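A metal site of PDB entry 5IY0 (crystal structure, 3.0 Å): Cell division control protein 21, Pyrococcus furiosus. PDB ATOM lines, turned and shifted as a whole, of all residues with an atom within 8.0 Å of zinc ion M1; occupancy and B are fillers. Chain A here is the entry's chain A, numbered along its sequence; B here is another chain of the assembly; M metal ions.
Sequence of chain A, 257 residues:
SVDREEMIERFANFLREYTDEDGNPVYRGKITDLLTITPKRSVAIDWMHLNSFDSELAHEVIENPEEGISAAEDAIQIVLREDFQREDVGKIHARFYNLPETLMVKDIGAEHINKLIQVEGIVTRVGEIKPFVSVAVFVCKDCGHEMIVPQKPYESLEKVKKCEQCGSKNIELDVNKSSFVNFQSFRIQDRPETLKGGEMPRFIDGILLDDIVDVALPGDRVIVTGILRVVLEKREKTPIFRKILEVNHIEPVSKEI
The side-chain hydroxyl (OG) of Ser 168 sits close to the side-chain sulfur (SG) of Cys 166 of chain A (3.2 Å). The backbone NH (N) of Gln 165 sits close to the side-chain sulfur (SG) of Cys 163 (3.5 Å). N of Cys 163 lies within hydrogen-bond range of O of Ser 168 (3.0 Å). The side-chain sulfur of Cys 140 sits close to the backbone NH of Asp 142 of chain A (3.5 Å). The side-chain sulfur (SG) of Cys 143 of chain A lies close to the backbone NH (N) of His 145 (3.7 Å). The side-chain sulfur (SG) of Cys 143 of chain A lies close to the side-chain amide oxygen (OE1) of Gln 165 (3.6 Å). SG of Cys 140 sits close to OG of Ser 168 (3.7 Å). The backbone NH of Cys 140 lies within hydrogen-bond range of the backbone carbonyl oxygen of His 145, at 3.0 Å.
Zinc ion M1 is bound by the side-chain sulfur (SG) of Cys 143 of chain A (2.2 Å). Zinc ion M1 is bound by the side-chain sulfur (SG) of Cys 166 of chain A (2.2 Å). Zinc ion M1 is bound by the side-chain sulfur (SG) of Cys 140 (2.4 Å). SG of Cys 163 binds zinc ion M1 (2.4 Å).
Of the 22 residues printed, 4 come within 4 Å of zinc ion M1.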
ATOM      1  N   VAL A 139     -27.986  19.088  14.601  1.00  0.00           N
ATOM      2  CA  VAL A 139     -26.823  19.951  14.821  1.00  0.00           C
ATOM      3  C   VAL A 139     -26.961  21.237  14.017  1.00  0.00           C
ATOM      4  O   VAL A 139     -27.332  21.208  12.840  1.00  0.00           O
ATOM      5  CB  VAL A 139     -25.509  19.232  14.466  1.00  0.00           C
ATOM      6  CG1 VAL A 139     -24.316  20.096  14.853  1.00  0.00           C
ATOM      7  CG2 VAL A 139     -25.419  17.897  15.188  1.00  0.00           C
ATOM      8  N   CYS A 140     -26.639  22.344  14.667  1.00  0.00           N
ATOM      9  CA  CYS A 140     -26.580  23.656  14.021  1.00  0.00           C
ATOM     10  C   CYS A 140     -25.232  23.837  13.358  1.00  0.00           C
ATOM     11  O   CYS A 140     -24.190  23.782  14.021  1.00  0.00           O
ATOM     12  CB  CYS A 140     -26.778  24.760  15.059  1.00  0.00           C
ATOM     13  SG  CYS A 140     -26.815  26.425  14.360  1.00  0.00           S
ATOM     14  N   LYS A 141     -25.246  24.087  12.053  1.00  0.00           N
ATOM     15  CA  LYS A 141     -23.999  24.242  11.293  1.00  0.00           C
ATOM     16  C   LYS A 141     -23.359  25.604  11.536  1.00  0.00           C
ATOM     17  O   LYS A 141     -22.168  25.800  11.268  1.00  0.00           O
ATOM     18  CB  LYS A 141     -24.257  24.093   9.797  1.00  0.00           C
ATOM     19  CG  LYS A 141     -24.935  22.804   9.380  1.00  0.00           C
ATOM     20  CD  LYS A 141     -25.170  22.811   7.884  1.00  0.00           C
ATOM     21  CE  LYS A 141     -26.068  21.666   7.467  1.00  0.00           C
ATOM     22  NZ  LYS A 141     -26.260  21.644   6.003  1.00  0.00           N
ATOM     23  N   ASP A 142     -24.155  26.550  12.034  1.00  0.00           N
ATOM     24  CA  ASP A 142     -23.686  27.916  12.280  1.00  0.00           C
ATOM     25  C   ASP A 142     -22.944  28.061  13.631  1.00  0.00           C
ATOM     26  O   ASP A 142     -21.998  28.843  13.700  1.00  0.00           O
ATOM     27  CB  ASP A 142     -24.876  28.901  12.182  1.00  0.00           C
ATOM     28  CG  ASP A 142     -25.486  28.960  10.755  1.00  0.00           C
ATOM     29  OD1 ASP A 142     -24.783  28.579   9.793  1.00  0.00           O
ATOM     30  OD2 ASP A 142     -26.661  29.383  10.596  1.00  0.00           O
ATOM     31  N   CYS A 143     -23.348  27.337  14.673  1.00  0.00           N
ATOM     32  CA  CYS A 143     -22.659  27.415  15.983  1.00  0.00           C
ATOM     33  C   CYS A 143     -22.291  26.078  16.637  1.00  0.00           C
ATOM     34  O   CYS A 143     -21.741  26.071  17.734  1.00  0.00           O
ATOM     35  CB  CYS A 143     -23.493  28.232  16.981  1.00  0.00           C
ATOM     36  SG  CYS A 143     -24.941  27.420  17.745  1.00  0.00           S
ATOM     37  N   GLY A 144     -22.582  24.954  15.978  1.00  0.00           N
ATOM     38  CA  GLY A 144     -22.232  23.628  16.502  1.00  0.00           C
ATOM     39  C   GLY A 144     -23.078  23.112  17.666  1.00  0.00           C
ATOM     40  O   GLY A 144     -22.815  22.018  18.192  1.00  0.00           O
ATOM     41  N   HIS A 145     -24.109  23.875  18.044  1.00  0.00           N
ATOM     42  CA  HIS A 145     -24.979  23.488  19.147  1.00  0.00           C
ATOM     43  C   HIS A 145     -25.859  22.304  18.754  1.00  0.00           C
ATOM     44  O   HIS A 145     -26.506  22.316  17.682  1.00  0.00           O
ATOM     45  CB  HIS A 145     -25.873  24.647  19.597  1.00  0.00           C
ATOM     46  CG  HIS A 145     -26.714  24.309  20.794  1.00  0.00           C
ATOM     47  ND1 HIS A 145     -28.088  24.480  20.824  1.00  0.00           N
ATOM     48  CD2 HIS A 145     -26.383  23.759  21.980  1.00  0.00           C
ATOM     49  CE1 HIS A 145     -28.551  24.082  21.987  1.00  0.00           C
ATOM     50  NE2 HIS A 145     -27.537  23.637  22.711  1.00  0.00           N
ATOM     51  N   GLU A 146     -25.887  21.315  19.640  1.00  0.00           N
ATOM     52  CA  GLU A 146     -26.625  20.079  19.432  1.00  0.00           C
ATOM     53  C   GLU A 146     -27.924  20.047  20.232  1.00  0.00           C
ATOM     54  O   GLU A 146     -27.930  20.384  21.407  1.00  0.00           O
ATOM     55  CB  GLU A 146     -25.744  18.893  19.823  1.00  0.00           C
ATOM     56  CG  GLU A 146     -24.459  18.796  19.012  1.00  0.00           C
ATOM     57  CD  GLU A 146     -23.676  17.516  19.299  1.00  0.00           C
ATOM     58  OE1 GLU A 146     -24.153  16.637  20.040  1.00  0.00           O
ATOM     59  OE2 GLU A 146     -22.553  17.388  18.767  1.00  0.00           O
ATOM     60  N   MET A 147     -29.002  19.600  19.604  1.00  0.00           N
ATOM     61  CA  MET A 147     -30.300  19.464  20.263  1.00  0.00           C
ATOM     62  C   MET A 147     -30.810  18.032  20.155  1.00  0.00           C
ATOM     63  O   MET A 147     -31.067  17.533  19.069  1.00  0.00           O
ATOM     64  CB  MET A 147     -31.302  20.405  19.623  1.00  0.00           C
ATOM     65  CG  MET A 147     -30.779  21.820  19.453  1.00  0.00           C
ATOM     66  SD  MET A 147     -31.955  22.876  18.613  1.00  0.00           S
ATOM     67  CE  MET A 147     -33.234  22.987  19.861  1.00  0.00           C
ATOM     68  N   LYS A 162     -35.173  25.812  14.424  1.00  0.00           N
ATOM     69  CA  LYS A 162     -34.359  26.944  14.845  1.00  0.00           C
ATOM     70  C   LYS A 162     -33.392  26.508  15.908  1.00  0.00           C
ATOM     71  O   LYS A 162     -33.783  25.869  16.886  1.00  0.00           O
ATOM     72  CB  LYS A 162     -35.237  28.068  15.404  1.00  0.00           C
ATOM     73  CG  LYS A 162     -35.690  29.049  14.331  1.00  0.00           C
ATOM     74  CD  LYS A 162     -36.350  30.306  14.863  1.00  0.00           C
ATOM     75  CE  LYS A 162     -36.857  31.135  13.685  1.00  0.00           C
ATOM     76  NZ  LYS A 162     -37.724  32.245  14.102  1.00  0.00           N
ATOM     77  N   CYS A 163     -32.124  26.834  15.727  1.00  0.00           N
ATOM     78  CA  CYS A 163     -31.142  26.598  16.774  1.00  0.00           C
ATOM     79  C   CYS A 163     -31.587  27.297  18.060  1.00  0.00           C
ATOM     80  O   CYS A 163     -31.780  28.507  18.104  1.00  0.00           O
ATOM     81  CB  CYS A 163     -29.746  27.062  16.350  1.00  0.00           C
ATOM     82  SG  CYS A 163     -28.477  26.698  17.580  1.00  0.00           S
ATOM     83  N   GLU A 164     -31.811  26.489  19.094  1.00  0.00           N
ATOM     84  CA  GLU A 164     -32.080  26.955  20.446  1.00  0.00           C
ATOM     85  C   GLU A 164     -31.202  28.130  20.859  1.00  0.00           C
ATOM     86  O   GLU A 164     -31.659  29.032  21.549  1.00  0.00           O
ATOM     87  CB  GLU A 164     -31.796  25.828  21.428  1.00  0.00           C
ATOM     88  CG  GLU A 164     -32.901  25.489  22.407  1.00  0.00           C
ATOM     89  CD  GLU A 164     -32.487  24.366  23.326  1.00  0.00           C
ATOM     90  OE1 GLU A 164     -33.195  24.128  24.332  1.00  0.00           O
ATOM     91  OE2 GLU A 164     -31.438  23.722  23.069  1.00  0.00           O
ATOM     92  N   GLN A 165     -29.932  28.070  20.453  1.00  0.00           N
ATOM     93  CA  GLN A 165     -28.912  29.044  20.861  1.00  0.00           C
ATOM     94  C   GLN A 165     -28.761  30.257  19.938  1.00  0.00           C
ATOM     95  O   GLN A 165     -28.919  31.386  20.385  1.00  0.00           O
ATOM     96  CB  GLN A 165     -27.575  28.346  20.967  1.00  0.00           C
ATOM     97  CG  GLN A 165     -26.557  29.093  21.795  1.00  0.00           C
ATOM     98  CD  GLN A 165     -25.399  28.196  22.131  1.00  0.00           C
ATOM     99  OE1 GLN A 165     -24.620  27.830  21.258  1.00  0.00           O
ATOM    100  NE2 GLN A 165     -25.297  27.815  23.392  1.00  0.00           N
ATOM    101  N   CYS A 166     -28.442  30.011  18.672  1.00  0.00           N
ATOM    102  CA  CYS A 166     -28.198  31.095  17.721  1.00  0.00           C
ATOM    103  C   CYS A 166     -29.451  31.553  16.971  1.00  0.00           C
ATOM    104  O   CYS A 166     -29.455  32.644  16.390  1.00  0.00           O
ATOM    105  CB  CYS A 166     -27.107  30.689  16.718  1.00  0.00           C
ATOM    106  SG  CYS A 166     -27.586  29.492  15.451  1.00  0.00           S
ATOM    107  N   GLY A 167     -30.497  30.727  16.959  1.00  0.00           N
ATOM    108  CA  GLY A 167     -31.753  31.060  16.280  1.00  0.00           C
ATOM    109  C   GLY A 167     -31.825  30.860  14.778  1.00  0.00           C
ATOM    110  O   GLY A 167     -32.887  31.080  14.189  1.00  0.00           O
ATOM    111  N   SER A 168     -30.724  30.448  14.134  1.00  0.00           N
ATOM    112  CA  SER A 168     -30.716  30.266  12.664  1.00  0.00           C
ATOM    113  C   SER A 168     -31.453  29.013  12.256  1.00  0.00           C
ATOM    114  O   SER A 168     -31.600  28.068  13.054  1.00  0.00           O
ATOM    115  CB  SER A 168     -29.284  30.195  12.113  1.00  0.00           C
ATOM    116  OG  SER A 168     -28.665  28.974  12.449  1.00  0.00           O
ATOM    117  N   LYS A 169     -31.900  29.000  10.998  1.00  0.00           N
ATOM    118  CA  LYS A 169     -32.636  27.875  10.421  1.00  0.00           C
ATOM    119  C   LYS A 169     -31.693  26.937   9.677  1.00  0.00           C
ATOM    120  O   LYS A 169     -32.142  26.197   8.800  1.00  0.00           O
ATOM    121  CB  LYS A 169     -33.742  28.371   9.483  1.00  0.00           C
ATOM    122  CG  LYS A 169     -34.677  29.377  10.106  1.00  0.00           C
ATOM    123  CD  LYS A 169     -35.397  30.203   9.061  1.00  0.00           C
ATOM    124  CE  LYS A 169     -36.031  31.431   9.686  1.00  0.00           C
ATOM    125  NZ  LYS A 169     -36.581  32.346   8.641  1.00  0.00           N
ATOM    126  N   ASN A 170     -30.423  26.965  10.033  1.00  0.00           N
ATOM    127  CA  ASN A 170     -29.400  26.120   9.405  1.00  0.00           C
ATOM    128  C   ASN A 170     -29.100  24.864  10.261  1.00  0.00           C
ATOM    129  O   ASN A 170     -27.952  24.592  10.669  1.00  0.00           O
ATOM    130  CB  ASN A 170     -28.140  26.960   9.166  1.00  0.00           C
ATOM    131  CG  ASN A 170     -27.395  26.511   7.940  1.00  0.00           C
ATOM    132  OD1 ASN A 170     -27.991  26.289   6.892  1.00  0.00           O
ATOM    133  ND2 ASN A 170     -26.085  26.386   8.043  1.00  0.00           N
ATOM    134  N   ILE A 171     -30.180  24.117  10.508  1.00  0.00           N
ATOM    135  CA  ILE A 171     -30.193  22.920  11.340  1.00  0.00           C
ATOM    136  C   ILE A 171     -30.507  21.706  10.456  1.00  0.00           C
ATOM    137  O   ILE A 171     -31.428  21.771   9.629  1.00  0.00           O
ATOM    138  CB  ILE A 171     -31.302  23.046  12.407  1.00  0.00           C
ATOM    139  CG1 ILE A 171     -30.889  23.972  13.563  1.00  0.00           C
ATOM    140  CG2 ILE A 171     -31.678  21.670  12.953  1.00  0.00           C
ATOM    141  CD1 ILE A 171     -30.107  23.309  14.684  1.00  0.00           C
ATOM    142  N   ASP B 142     -23.932  34.566  20.772  1.00  0.00           N
ATOM    143  CA  ASP B 142     -24.578  33.304  20.445  1.00  0.00           C
ATOM    144  C   ASP B 142     -23.584  32.235  19.939  1.00  0.00           C
ATOM    145  O   ASP B 142     -23.777  31.059  20.222  1.00  0.00           O
ATOM    146  CB  ASP B 142     -25.720  33.548  19.432  1.00  0.00           C
ATOM    147  CG  ASP B 142     -26.869  34.409  20.009  1.00  0.00           C
ATOM    148  OD1 ASP B 142     -26.979  34.492  21.250  1.00  0.00           O
ATOM    149  OD2 ASP B 142     -27.675  34.999  19.242  1.00  0.00           O
ATOM    150  N   CYS B 143     -22.540  32.626  19.194  1.00  0.00           N
ATOM    151  CA  CYS B 143     -21.530  31.664  18.694  1.00  0.00           C
ATOM    152  C   CYS B 143     -20.051  32.024  18.928  1.00  0.00           C
ATOM    153  O   CYS B 143     -19.159  31.279  18.503  1.00  0.00           O
ATOM    154  CB  CYS B 143     -21.753  31.391  17.195  1.00  0.00           C
ATOM    155  SG  CYS B 143     -21.212  32.677  16.030  1.00  0.00           S
ATOM    156  N   CYS B 166     -23.504  33.167  12.260  1.00  0.00           N
ATOM    157  CA  CYS B 166     -24.795  32.632  12.719  1.00  0.00           C
ATOM    158  C   CYS B 166     -25.991  33.469  12.267  1.00  0.00           C
ATOM    159  O   CYS B 166     -27.126  32.981  12.275  1.00  0.00           O
ATOM    160  CB  CYS B 166     -24.807  32.441  14.246  1.00  0.00           C
ATOM    161  SG  CYS B 166     -24.966  33.940  15.256  1.00  0.00           S
HETATM  162 ZN    ZN M   1     -26.625  27.695  16.358  1.00  0.00          ZN
HETATM  163 ZN    ZN M   2     -22.939  34.225  15.904  1.00  0.00          ZN
